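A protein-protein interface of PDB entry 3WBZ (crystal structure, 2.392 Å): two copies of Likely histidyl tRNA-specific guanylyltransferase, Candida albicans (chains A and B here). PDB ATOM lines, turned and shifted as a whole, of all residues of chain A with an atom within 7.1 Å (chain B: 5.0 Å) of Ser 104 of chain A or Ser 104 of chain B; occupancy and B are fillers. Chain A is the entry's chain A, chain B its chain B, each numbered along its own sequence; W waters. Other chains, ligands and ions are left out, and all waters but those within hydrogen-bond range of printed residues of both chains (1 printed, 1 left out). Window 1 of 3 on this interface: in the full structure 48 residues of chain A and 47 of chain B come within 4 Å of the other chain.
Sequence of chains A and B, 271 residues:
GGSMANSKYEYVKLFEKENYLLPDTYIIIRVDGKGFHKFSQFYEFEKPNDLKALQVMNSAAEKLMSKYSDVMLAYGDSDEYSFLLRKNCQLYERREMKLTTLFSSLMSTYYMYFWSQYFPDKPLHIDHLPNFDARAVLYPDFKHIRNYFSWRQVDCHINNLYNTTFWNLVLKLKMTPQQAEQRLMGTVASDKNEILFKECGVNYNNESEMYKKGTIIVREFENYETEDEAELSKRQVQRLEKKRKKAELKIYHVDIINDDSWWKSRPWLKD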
ATOM      1  N   ILE A  29      22.363 -35.026  17.956  1.00  0.00           N
ATOM      2  CA  ILE A  29      22.802 -33.744  17.402  1.00  0.00           C
ATOM      3  C   ILE A  29      21.580 -32.919  17.114  1.00  0.00           C
ATOM      4  O   ILE A  29      20.689 -33.341  16.373  1.00  0.00           O
ATOM      5  CB  ILE A  29      23.649 -33.928  16.140  1.00  0.00           C
ATOM      6  CG1 ILE A  29      24.901 -34.727  16.512  1.00  0.00           C
ATOM      7  CG2 ILE A  29      24.027 -32.545  15.513  1.00  0.00           C
ATOM      8  CD1 ILE A  29      25.720 -35.078  15.344  1.00  0.00           C
ATOM      9  N   VAL A  31      20.148 -29.343  15.661  1.00  0.00           N
ATOM     10  CA  VAL A  31      20.431 -28.088  14.961  1.00  0.00           C
ATOM     11  C   VAL A  31      19.229 -27.163  15.028  1.00  0.00           C
ATOM     12  O   VAL A  31      18.086 -27.605  14.991  1.00  0.00           O
ATOM     13  CB  VAL A  31      20.854 -28.340  13.484  1.00  0.00           C
ATOM     14  CG1 VAL A  31      21.967 -29.368  13.436  1.00  0.00           C
ATOM     15  CG2 VAL A  31      19.677 -28.797  12.629  1.00  0.00           C
ATOM     16  N   LEU A  64      20.376 -35.375   4.585  1.00  0.00           N
ATOM     17  CA  LEU A  64      21.481 -35.587   5.517  1.00  0.00           C
ATOM     18  C   LEU A  64      21.450 -37.014   6.050  1.00  0.00           C
ATOM     19  O   LEU A  64      22.451 -37.726   6.056  1.00  0.00           O
ATOM     20  CB  LEU A  64      21.414 -34.574   6.677  1.00  0.00           C
ATOM     21  CG  LEU A  64      22.548 -34.520   7.717  1.00  0.00           C
ATOM     22  CD1 LEU A  64      22.594 -33.192   8.420  1.00  0.00           C
ATOM     23  CD2 LEU A  64      22.405 -35.640   8.754  1.00  0.00           C
ATOM     24  N   MET A  97      33.903 -31.692  17.414  1.00  0.00           N
ATOM     25  CA  MET A  97      34.080 -30.605  16.449  1.00  0.00           C
ATOM     26  C   MET A  97      33.630 -31.014  15.052  1.00  0.00           C
ATOM     27  O   MET A  97      32.909 -30.266  14.400  1.00  0.00           O
ATOM     28  CB  MET A  97      35.548 -30.153  16.413  1.00  0.00           C
ATOM     29  CG  MET A  97      35.896 -29.119  15.329  1.00  0.00           C
ATOM     30  SD  MET A  97      36.414 -29.717  13.658  1.00  0.00           S
ATOM     31  CE  MET A  97      37.951 -30.575  14.081  1.00  0.00           C
ATOM     32  N   LYS A  98      34.027 -32.204  14.602  1.00  0.00           N
ATOM     33  CA  LYS A  98      33.655 -32.680  13.266  1.00  0.00           C
ATOM     34  C   LYS A  98      32.164 -32.939  13.148  1.00  0.00           C
ATOM     35  O   LYS A  98      31.525 -32.499  12.204  1.00  0.00           O
ATOM     36  CB  LYS A  98      34.405 -33.965  12.915  1.00  0.00           C
ATOM     37  CG  LYS A  98      35.894 -33.786  12.663  1.00  0.00           C
ATOM     38  CD  LYS A  98      36.172 -33.106  11.352  1.00  0.00           C
ATOM     39  CE  LYS A  98      37.668 -33.057  11.083  1.00  0.00           C
ATOM     40  NZ  LYS A  98      37.965 -32.415   9.770  1.00  0.00           N
ATOM     41  N   LEU A  99      31.603 -33.659  14.109  1.00  0.00           N
ATOM     42  CA  LEU A  99      30.194 -34.013  14.034  1.00  0.00           C
ATOM     43  C   LEU A  99      29.312 -32.764  14.010  1.00  0.00           C
ATOM     44  O   LEU A  99      28.416 -32.645  13.158  1.00  0.00           O
ATOM     45  CB  LEU A  99      29.816 -34.891  15.216  1.00  0.00           C
ATOM     46  CG  LEU A  99      30.328 -36.321  15.168  1.00  0.00           C
ATOM     47  CD1 LEU A  99      30.036 -36.998  16.498  1.00  0.00           C
ATOM     48  CD2 LEU A  99      29.586 -37.032  14.039  1.00  0.00           C
ATOM     49  N   THR A 100      29.588 -31.814  14.904  1.00  0.00           N
ATOM     50  CA  THR A 100      28.707 -30.658  15.019  1.00  0.00           C
ATOM     51  C   THR A 100      28.908 -29.645  13.858  1.00  0.00           C
ATOM     52  O   THR A 100      27.937 -29.207  13.270  1.00  0.00           O
ATOM     53  CB  THR A 100      28.886 -29.931  16.405  1.00  0.00           C
ATOM     54  OG1 THR A 100      30.257 -29.576  16.621  1.00  0.00           O
ATOM     55  CG2 THR A 100      28.419 -30.846  17.548  1.00  0.00           C
ATOM     56  N   THR A 101      30.146 -29.323  13.479  1.00  0.00           N
ATOM     57  CA  THR A 101      30.308 -28.277  12.471  1.00  0.00           C
ATOM     58  C   THR A 101      29.937 -28.788  11.087  1.00  0.00           C
ATOM     59  O   THR A 101      29.455 -28.019  10.270  1.00  0.00           O
ATOM     60  CB  THR A 101      31.752 -27.688  12.424  1.00  0.00           C
ATOM     61  OG1 THR A 101      32.698 -28.699  12.047  1.00  0.00           O
ATOM     62  CG2 THR A 101      32.135 -27.053  13.772  1.00  0.00           C
ATOM     63  N   LEU A 102      30.062 -30.094  10.862  1.00  0.00           N
ATOM     64  CA  LEU A 102      29.592 -30.679   9.604  1.00  0.00           C
ATOM     65  C   LEU A 102      28.074 -30.738   9.569  1.00  0.00           C
ATOM     66  O   LEU A 102      27.467 -30.509   8.510  1.00  0.00           O
ATOM     67  CB  LEU A 102      30.214 -32.051   9.361  1.00  0.00           C
ATOM     68  CG  LEU A 102      31.667 -31.779   8.916  1.00  0.00           C
ATOM     69  CD1 LEU A 102      32.543 -33.049   8.853  1.00  0.00           C
ATOM     70  CD2 LEU A 102      31.722 -31.005   7.566  1.00  0.00           C
ATOM     71  N   PHE A 103      27.439 -31.057  10.695  1.00  0.00           N
ATOM     72  CA  PHE A 103      25.976 -31.068  10.687  1.00  0.00           C
ATOM     73  C   PHE A 103      25.371 -29.669  10.452  1.00  0.00           C
ATOM     74  O   PHE A 103      24.484 -29.544   9.620  1.00  0.00           O
ATOM     75  CB  PHE A 103      25.434 -31.685  11.979  1.00  0.00           C
ATOM     76  CG  PHE A 103      25.143 -33.162  11.846  1.00  0.00           C
ATOM     77  CD1 PHE A 103      26.167 -34.065  11.563  1.00  0.00           C
ATOM     78  CD2 PHE A 103      23.852 -33.655  12.020  1.00  0.00           C
ATOM     79  CE1 PHE A 103      25.903 -35.433  11.416  1.00  0.00           C
ATOM     80  CE2 PHE A 103      23.583 -35.019  11.898  1.00  0.00           C
ATOM     81  CZ  PHE A 103      24.601 -35.907  11.595  1.00  0.00           C
ATOM     82  N   SER A 104      25.889 -28.620  11.093  1.00  0.00           N
ATOM     83  CA  SER A 104      25.338 -27.286  10.894  1.00  0.00           C
ATOM     84  C   SER A 104      25.640 -26.793   9.462  1.00  0.00           C
ATOM     85  O   SER A 104      24.847 -26.078   8.856  1.00  0.00           O
ATOM     86  CB  SER A 104      25.897 -26.310  11.932  1.00  0.00           C
ATOM     87  OG  SER A 104      27.263 -26.040  11.690  1.00  0.00           O
ATOM     88  N   SER A 105      26.794 -27.199   8.941  1.00  0.00           N
ATOM     89  CA  SER A 105      27.190 -26.889   7.575  1.00  0.00           C
ATOM     90  C   SER A 105      26.252 -27.587   6.575  1.00  0.00           C
ATOM     91  O   SER A 105      25.689 -26.935   5.681  1.00  0.00           O
ATOM     92  CB  SER A 105      28.651 -27.313   7.366  1.00  0.00           C
ATOM     93  OG  SER A 105      29.096 -27.139   6.048  1.00  0.00           O
ATOM     94  N   LEU A 106      26.025 -28.886   6.779  1.00  0.00           N
ATOM     95  CA  LEU A 106      25.146 -29.686   5.914  1.00  0.00           C
ATOM     96  C   LEU A 106      23.707 -29.181   5.906  1.00  0.00           C
ATOM     97  O   LEU A 106      23.100 -29.063   4.846  1.00  0.00           O
ATOM     98  CB  LEU A 106      25.154 -31.141   6.356  1.00  0.00           C
ATOM     99  CG  LEU A 106      26.407 -31.925   5.948  1.00  0.00           C
ATOM    100  CD1 LEU A 106      26.458 -33.221   6.758  1.00  0.00           C
ATOM    101  CD2 LEU A 106      26.492 -32.207   4.461  1.00  0.00           C
ATOM    102  N   MET A 107      23.141 -28.922   7.085  1.00  0.00           N
ATOM    103  CA  MET A 107      21.767 -28.444   7.144  1.00  0.00           C
ATOM    104  C   MET A 107      21.670 -27.088   6.459  1.00  0.00           C
ATOM    105  O   MET A 107      20.704 -26.827   5.747  1.00  0.00           O
ATOM    106  CB  MET A 107      21.273 -28.337   8.595  1.00  0.00           C
ATOM    107  CG  MET A 107      20.864 -29.673   9.218  1.00  0.00           C
ATOM    108  SD  MET A 107      19.539 -30.480   8.298  1.00  0.00           S
ATOM    109  CE  MET A 107      18.216 -29.295   8.593  1.00  0.00           C
ATOM    110  N   SER A 108      22.690 -26.249   6.646  1.00  0.00           N
ATOM    111  CA  SER A 108      22.706 -24.918   6.046  1.00  0.00           C
ATOM    112  C   SER A 108      22.672 -24.957   4.523  1.00  0.00           C
ATOM    113  O   SER A 108      21.887 -24.242   3.907  1.00  0.00           O
ATOM    114  CB  SER A 108      23.943 -24.147   6.482  1.00  0.00           C
ATOM    115  OG  SER A 108      23.893 -23.845   7.858  1.00  0.00           O
ATOM    116  N   THR A 109      23.534 -25.786   3.934  1.00  0.00           N
ATOM    117  CA  THR A 109      23.664 -25.839   2.480  1.00  0.00           C
ATOM    118  C   THR A 109      22.504 -26.591   1.855  1.00  0.00           C
ATOM    119  O   THR A 109      22.008 -26.183   0.805  1.00  0.00           O
ATOM    120  CB  THR A 109      25.017 -26.460   2.028  1.00  0.00           C
ATOM    121  OG1 THR A 109      25.209 -27.777   2.578  1.00  0.00           O
ATOM    122  CG2 THR A 109      26.163 -25.564   2.438  1.00  0.00           C
ATOM    123  N   PRO A 130      20.280 -18.719   5.505  1.00  0.00           N
ATOM    124  CA  PRO A 130      19.856 -19.618   6.580  1.00  0.00           C
ATOM    125  C   PRO A 130      21.040 -20.280   7.284  1.00  0.00           C
ATOM    126  O   PRO A 130      21.725 -21.119   6.698  1.00  0.00           O
ATOM    127  CB  PRO A 130      19.014 -20.665   5.853  1.00  0.00           C
ATOM    128  CG  PRO A 130      19.635 -20.728   4.484  1.00  0.00           C
ATOM    129  CD  PRO A 130      20.091 -19.323   4.174  1.00  0.00           C
ATOM    130  N   ASN A 131      21.283 -19.885   8.528  1.00  0.00           N
ATOM    131  CA  ASN A 131      22.367 -20.465   9.301  1.00  0.00           C
ATOM    132  C   ASN A 131      21.838 -21.294  10.455  1.00  0.00           C
ATOM    133  O   ASN A 131      20.724 -21.059  10.937  1.00  0.00           O
ATOM    134  CB  ASN A 131      23.279 -19.367   9.798  1.00  0.00           C
ATOM    135  CG  ASN A 131      23.929 -18.609   8.653  1.00  0.00           C
ATOM    136  OD1 ASN A 131      23.718 -17.408   8.493  1.00  0.00           O
ATOM    137  ND2 ASN A 131      24.703 -19.312   7.841  1.00  0.00           N
ATOM    138  N   PHE A 132      22.618 -22.295  10.859  1.00  0.00           N
ATOM    139  CA  PHE A 132      22.219 -23.194  11.935  1.00  0.00           C
ATOM    140  C   PHE A 132      23.352 -23.368  12.918  1.00  0.00           C
ATOM    141  O   PHE A 132      24.512 -23.410  12.510  1.00  0.00           O
ATOM    142  CB  PHE A 132      21.819 -24.557  11.381  1.00  0.00           C
ATOM    143  CG  PHE A 132      20.555 -24.541  10.608  1.00  0.00           C
ATOM    144  CD1 PHE A 132      20.553 -24.168   9.263  1.00  0.00           C
ATOM    145  CD2 PHE A 132      19.363 -24.932  11.208  1.00  0.00           C
ATOM    146  CE1 PHE A 132      19.383 -24.146   8.537  1.00  0.00           C
ATOM    147  CE2 PHE A 132      18.168 -24.919  10.489  1.00  0.00           C
ATOM    148  CZ  PHE A 132      18.177 -24.513   9.139  1.00  0.00           C
ATOM    149  N   ASP A 133      23.035 -23.485  14.208  1.00  0.00           N
ATOM    150  CA  ASP A 133      24.029 -23.949  15.161  1.00  0.00           C
ATOM    151  C   ASP A 133      23.875 -25.475  15.177  1.00  0.00           C
ATOM    152  O   ASP A 133      23.008 -26.029  14.496  1.00  0.00           O
ATOM    153  CB  ASP A 133      23.830 -23.304  16.544  1.00  0.00           C
ATOM    154  CG  ASP A 133      22.707 -23.939  17.363  1.00  0.00           C
ATOM    155  OD1 ASP A 133      21.880 -24.748  16.855  1.00  0.00           O
ATOM    156  OD2 ASP A 133      22.614 -23.574  18.557  1.00  0.00           O
ATOM    157  N   ALA A 134      24.714 -26.164  15.924  1.00  0.00           N
ATOM    158  CA  ALA A 134      24.548 -27.606  16.106  1.00  0.00           C
ATOM    159  C   ALA A 134      25.244 -27.955  17.390  1.00  0.00           C
ATOM    160  O   ALA A 134      26.310 -27.427  17.655  1.00  0.00           O
ATOM    161  CB  ALA A 134      25.141 -28.419  14.906  1.00  0.00           C
ATOM    162  N   ARG A 135      24.625 -28.798  18.205  1.00  0.00           N
ATOM    163  CA  ARG A 135      25.269 -29.270  19.435  1.00  0.00           C
ATOM    164  C   ARG A 135      25.116 -30.772  19.531  1.00  0.00           C
ATOM    165  O   ARG A 135      24.156 -31.338  19.037  1.00  0.00           O
ATOM    166  CB  ARG A 135      24.681 -28.596  20.683  1.00  0.00           C
ATOM    167  CG  ARG A 135      23.262 -29.064  21.018  1.00  0.00           C
ATOM    168  CD  ARG A 135      22.619 -28.122  22.005  1.00  0.00           C
ATOM    169  NE  ARG A 135      22.353 -26.835  21.376  1.00  0.00           N
ATOM    170  CZ  ARG A 135      22.179 -25.695  22.036  1.00  0.00           C
ATOM    171  NH1 ARG A 135      22.242 -25.674  23.359  1.00  0.00           N
ATOM    172  NH2 ARG A 135      21.939 -24.574  21.367  1.00  0.00           N
ATOM    173  N   VAL B  31      38.474 -22.955   9.160  1.00  0.00           N
ATOM    174  CA  VAL B  31      37.514 -23.766   8.408  1.00  0.00           C
ATOM    175  C   VAL B  31      38.229 -24.424   7.252  1.00  0.00           C
ATOM    176  O   VAL B  31      39.207 -23.903   6.728  1.00  0.00           O
ATOM    177  CB  VAL B  31      36.317 -22.945   7.890  1.00  0.00           C
ATOM    178  CG1 VAL B  31      35.670 -22.133   9.049  1.00  0.00           C
ATOM    179  CG2 VAL B  31      36.748 -22.018   6.741  1.00  0.00           C
ATOM    180  N   THR B 100      32.029 -22.209  16.512  1.00  0.00           N
ATOM    181  CA  THR B 100      32.518 -23.057  15.456  1.00  0.00           C
ATOM    182  C   THR B 100      31.383 -23.438  14.496  1.00  0.00           C
ATOM    183  O   THR B 100      31.586 -23.433  13.284  1.00  0.00           O
ATOM    184  CB  THR B 100      33.181 -24.301  16.020  1.00  0.00           C
ATOM    185  OG1 THR B 100      32.258 -25.001  16.862  1.00  0.00           O
ATOM    186  CG2 THR B 100      34.400 -23.905  16.814  1.00  0.00           C
ATOM    187  N   THR B 101      30.195 -23.757  15.018  1.00  0.00           N
ATOM    188  CA  THR B 101      29.120 -24.180  14.119  1.00  0.00           C
ATOM    189  C   THR B 101      28.561 -22.978  13.383  1.00  0.00           C
ATOM    190  O   THR B 101      28.083 -23.108  12.262  1.00  0.00           O
ATOM    191  CB  THR B 101      27.971 -24.912  14.857  1.00  0.00           C
ATOM    192  OG1 THR B 101      27.377 -24.035  15.836  1.00  0.00           O
ATOM    193  CG2 THR B 101      28.487 -26.159  15.529  1.00  0.00           C
ATOM    194  N   LEU B 102      28.693 -21.795  13.968  1.00  0.00           N
ATOM    195  CA  LEU B 102      28.276 -20.596  13.274  1.00  0.00           C
ATOM    196  C   LEU B 102      29.227 -20.324  12.109  1.00  0.00           C
ATOM    197  O   LEU B 102      28.784 -20.123  10.986  1.00  0.00           O
ATOM    198  CB  LEU B 102      28.269 -19.389  14.214  1.00  0.00           C
ATOM    199  CG  LEU B 102      28.212 -18.012  13.529  1.00  0.00           C
ATOM    200  CD1 LEU B 102      26.760 -17.643  13.227  1.00  0.00           C
ATOM    201  CD2 LEU B 102      28.877 -16.887  14.352  1.00  0.00           C
ATOM    202  N   PHE B 103      30.531 -20.414  12.359  1.00  0.00           N
ATOM    203  CA  PHE B 103      31.498 -20.183  11.299  1.00  0.00           C
ATOM    204  C   PHE B 103      31.404 -21.209  10.161  1.00  0.00           C
ATOM    205  O   PHE B 103      31.536 -20.830   8.988  1.00  0.00           O
ATOM    206  CB  PHE B 103      32.925 -20.182  11.852  1.00  0.00           C
ATOM    207  CG  PHE B 103      33.417 -18.817  12.246  1.00  0.00           C
ATOM    208  CD1 PHE B 103      32.863 -18.163  13.328  1.00  0.00           C
ATOM    209  CD2 PHE B 103      34.406 -18.182  11.504  1.00  0.00           C
ATOM    210  CE1 PHE B 103      33.292 -16.896  13.698  1.00  0.00           C
ATOM    211  CE2 PHE B 103      34.845 -16.913  11.847  1.00  0.00           C
ATOM    212  CZ  PHE B 103      34.288 -16.256  12.959  1.00  0.00           C
ATOM    213  N   SER B 104      31.174 -22.486  10.470  1.00  0.00           N
ATOM    214  CA  SER B 104      31.113 -23.476   9.393  1.00  0.00           C
ATOM    215  C   SER B 104      29.840 -23.273   8.569  1.00  0.00           C
ATOM    216  O   SER B 104      29.833 -23.418   7.360  1.00  0.00           O
ATOM    217  CB  SER B 104      31.193 -24.912   9.939  1.00  0.00           C
ATOM    218  OG  SER B 104      30.009 -25.273  10.599  1.00  0.00           O
ATOM    219  N   SER B 105      28.774 -22.907   9.250  1.00  0.00           N
ATOM    220  CA  SER B 105      27.516 -22.570   8.624  1.00  0.00           C
ATOM    221  C   SER B 105      27.639 -21.279   7.794  1.00  0.00           C
ATOM    222  O   SER B 105      27.176 -21.231   6.651  1.00  0.00           O
ATOM    223  CB  SER B 105      26.433 -22.424   9.693  1.00  0.00           C
ATOM    224  OG  SER B 105      25.235 -21.940   9.125  1.00  0.00           O
ATOM    225  N   LEU B 106      28.260 -20.244   8.363  1.00  0.00           N
ATOM    226  CA  LEU B 106      28.454 -18.987   7.643  1.00  0.00           C
ATOM    227  C   LEU B 106      29.315 -19.145   6.361  1.00  0.00           C
ATOM    228  O   LEU B 106      28.916 -18.660   5.300  1.00  0.00           O
ATOM    229  CB  LEU B 106      29.110 -17.936   8.531  1.00  0.00           C
ATOM    230  CG  LEU B 106      28.328 -17.175   9.607  1.00  0.00           C
ATOM    231  CD1 LEU B 106      29.339 -16.399  10.454  1.00  0.00           C
ATOM    232  CD2 LEU B 106      27.210 -16.272   9.098  1.00  0.00           C
ATOM    233  N   MET B 107      30.478 -19.801   6.458  1.00  0.00           N
ATOM    234  CA  MET B 107      31.338 -19.996   5.274  1.00  0.00           C
ATOM    235  C   MET B 107      30.647 -20.836   4.224  1.00  0.00           C
ATOM    236  O   MET B 107      30.784 -20.565   3.046  1.00  0.00           O
ATOM    237  CB  MET B 107      32.688 -20.637   5.613  1.00  0.00           C
ATOM    238  CG  MET B 107      33.734 -19.643   6.099  1.00  0.00           C
ATOM    239  SD  MET B 107      34.166 -18.342   4.909  1.00  0.00           S
ATOM    240  CE  MET B 107      35.086 -19.248   3.691  1.00  0.00           C
ATOM    241  N   SER B 108      29.892 -21.837   4.651  1.00  0.00           N
ATOM    242  CA  SER B 108      29.174 -22.708   3.722  1.00  0.00           C
ATOM    243  C   SER B 108      28.153 -21.965   2.866  1.00  0.00           C
ATOM    244  O   SER B 108      28.118 -22.113   1.647  1.00  0.00           O
ATOM    245  CB  SER B 108      28.454 -23.821   4.494  1.00  0.00           C
ATOM    246  OG  SER B 108      29.391 -24.714   5.067  1.00  0.00           O
ATOM    247  N   PHE B 132      31.941 -27.102   5.069  1.00  0.00           N
ATOM    248  CA  PHE B 132      33.151 -26.770   5.813  1.00  0.00           C
ATOM    249  C   PHE B 132      33.109 -27.350   7.221  1.00  0.00           C
ATOM    250  O   PHE B 132      32.041 -27.459   7.833  1.00  0.00           O
ATOM    251  CB  PHE B 132      33.334 -25.244   5.880  1.00  0.00           C
ATOM    252  CG  PHE B 132      33.686 -24.610   4.549  1.00  0.00           C
ATOM    253  CD1 PHE B 132      32.700 -24.285   3.629  1.00  0.00           C
ATOM    254  CD2 PHE B 132      35.007 -24.317   4.228  1.00  0.00           C
ATOM    255  CE1 PHE B 132      33.023 -23.699   2.416  1.00  0.00           C
ATOM    256  CE2 PHE B 132      35.333 -23.728   3.012  1.00  0.00           C
ATOM    257  CZ  PHE B 132      34.340 -23.434   2.104  1.00  0.00           C
ATOM    258  N   ASP B 133      34.262 -27.752   7.741  1.00  0.00           N
ATOM    259  CA  ASP B 133      34.345 -28.016   9.167  1.00  0.00           C
ATOM    260  C   ASP B 133      34.778 -26.693   9.809  1.00  0.00           C
ATOM    261  O   ASP B 133      35.029 -25.713   9.094  1.00  0.00           O
ATOM    262  CB  ASP B 133      35.307 -29.166   9.466  1.00  0.00           C
ATOM    263  CG  ASP B 133      36.778 -28.755   9.398  1.00  0.00           C
ATOM    264  OD1 ASP B 133      37.112 -27.656   8.900  1.00  0.00           O
ATOM    265  OD2 ASP B 133      37.631 -29.563   9.837  1.00  0.00           O
ATOM    266  N   ALA B 134      34.872 -26.651  11.133  1.00  0.00           N
ATOM    267  CA  ALA B 134      35.438 -25.473  11.789  1.00  0.00           C
ATOM    268  C   ALA B 134      35.947 -25.839  13.183  1.00  0.00           C
ATOM    269  O   ALA B 134      35.253 -26.480  13.957  1.00  0.00           O
ATOM    270  CB  ALA B 134      34.401 -24.338  11.868  1.00  0.00           C
HETATM  271  O   HOH W   1      31.530 -27.756  17.615  1.00  0.00           O
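NZ of Lys 98 of chain A is in salt-bridge range of OD2 of Asp 133 of chain B, 2.9 Å away.
O of Thr 101 of chain A sits at hydrogen-bond distance from OG of Ser 104 of chain B.
The side-chain hydroxyl (OG1) of Thr 101 of chain A sits at hydrogen-bond distance from the backbone NH (N) of Ala 134 of chain B (3.1 Å).
OG of Ser 104 of chain A lies within hydrogen-bond range of O of Thr 101 of chain B (3.1 Å).
The side-chain hydroxyl of Ser 104 of chain B lies within hydrogen-bond range of the side-chain hydroxyl of Ser 104 of chain A (3.1 Å).
The side-chain hydroxyl (OG) of Ser 108 of chain B sits at hydrogen-bond distance from the side-chain hydroxyl (OG) of Ser 105 of chain A (2.6 Å).
The side-chain hydroxyl (OG) of Ser 105 of chain A sits at hydrogen-bond distance from the backbone NH (N) of Phe 132 of chain B, 3.0 Å away.
The side-chain hydroxyl (OG) of Ser 108 of chain A is in hydrogen-bond range of the side-chain hydroxyl (OG) of Ser 105 of chain B, 2.7 Å away.
ND2 of Asn 131 of chain A lies within hydrogen-bond range of OG of Ser 105 of chain B, at 3.0 Å.
N of Phe 132 of chain A lies within hydrogen-bond range of OG of Ser 105 of chain B (3.2 Å).
The backbone NH (N) of Ala 134 of chain A is in hydrogen-bond range of the side-chain hydroxyl (OG1) of Thr 101 of chain B (3.4 Å).
The backbone carbonyl oxygen (O) of Ala 134 of chain B lies close to the side-chain sulfur (SD) of Met 97 of chain A (3.5 Å).
The backbone carbonyl oxygen (O) of Met 97 of chain A lies within hydrogen-bond range of the side-chain hydroxyl (OG1) of Thr 101 of chain A (2.8 Å).
The backbone carbonyl oxygen of Ser 105 of chain A sits at hydrogen-bond distance from the side-chain hydroxyl of Thr 109 of chain A, 3.3 Å away.
OG1 of Thr 109 of chain A sits at hydrogen-bond distance from O of Leu 106 of chain A.
The backbone carbonyl oxygen (O) of Thr 101 of chain B sits at hydrogen-bond distance from the side-chain hydroxyl (OG) of Ser 104 of chain B (3.3 Å).
O of Ser 104 of chain B is in hydrogen-bond range of OG of Ser 108 of chain B, at 2.7 Å.
The side-chain hydroxyl (OG) of Ser 108 of chain B sits at hydrogen-bond distance from the backbone NH (N) of Phe 132 of chain B.
Among the printed residues, pairs that only touch across the chains: Thr 101 of chain A with Asp 133 of chain B (3.4 Å), Asp 133 of chain A with Thr 101 of chain B (3.4 Å), Thr 109 of chain A with Ser 108 of chain B (3.5 Å), Leu 102 of chain A with Phe 132 of chain B (3.6 Å), Phe 132 of chain A with Thr 101 of chain B (3.6 Å), Thr 101 of chain A with Phe 132 of chain B (3.6 Å), Thr 101 of chain A with Thr 100 of chain B (3.7 Å), Asn 131 of chain A with Leu 106 of chain B (3.7 Å) and Thr 100 of chain A with Thr 101 of chain B (3.8 Å).
Of chain B, only Thr 101 (3.1 Å) and Ser 104 (3.1 Å) come within 4 Å of Ser 104 of chain A.
Printed residues of chain A within 4 Å of Ser 104 of chain B: Thr 101 and Ser 104.
Of the printed residues of chain A, Thr 100 of chain B touches Thr 101.
Of the printed residues of chain A, Ser 105 of chain B touches Ser 108, Asn 131 and Phe 132.
Printed residues of chain B within 4 Å of Thr 101 of chain A: Thr 100 (3.7 Å), Ser 104 (2.8 Å), Phe 132 (3.6 Å), Asp 133 (3.4 Å) and Ala 134 (3.1 Å).
Pro 130 of chain A touches none of the printed residues of chain B.
The nearest printed residue of chain A that does not touch Ser 104 of chain B is Ser 105 of chain A (4.01 Å).
The nearest printed residue of chain A that does not touch Asp 133 of chain B is Met 97 of chain A (4.01 Å).
Printed residues of chain B that touch a printed residue of chain A: Thr 100, Thr 101, Ser 104, Ser 105, Leu 106, Ser 108, Phe 132, Asp 133 and Ala 134.
Hydrophobic or aromatic side chains of chain A within 4 Å of the printed part of chain B: Met 97 and Leu 102.
Among the printed residues, Asp or Glu carboxylates within 4 Å of a Lys or Arg side-chain nitrogen of the other chain: Lys 98 of chain A with Asp 133 of chain B.
Thr 100 of chain A touches Thr 101 of chain B, and with the chains exchanged Thr 101 of chain A touches Thr 100 of chain B.
Thr 101 of chain A touches Ser 104 of chain B, and with the chains exchanged Ser 104 of chain A touches Thr 101 of chain B.
Thr 101 of chain A touches Ala 134 of chain B, and with the chains exchanged Ala 134 of chain A touches Thr 101 of chain B.
Ser 105 of chain A touches Phe 132 of chain B, and with the chains exchanged Phe 132 of chain A touches Ser 105 of chain B.
13 positions are printed for both chains.
Water W1 lies within hydrogen-bond range of the side-chain hydroxyl (OG1) of Thr 100 of chain A (2.4 Å) and the side-chain hydroxyl (OG1) of Thr 100 of chain B (2.9 Å).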
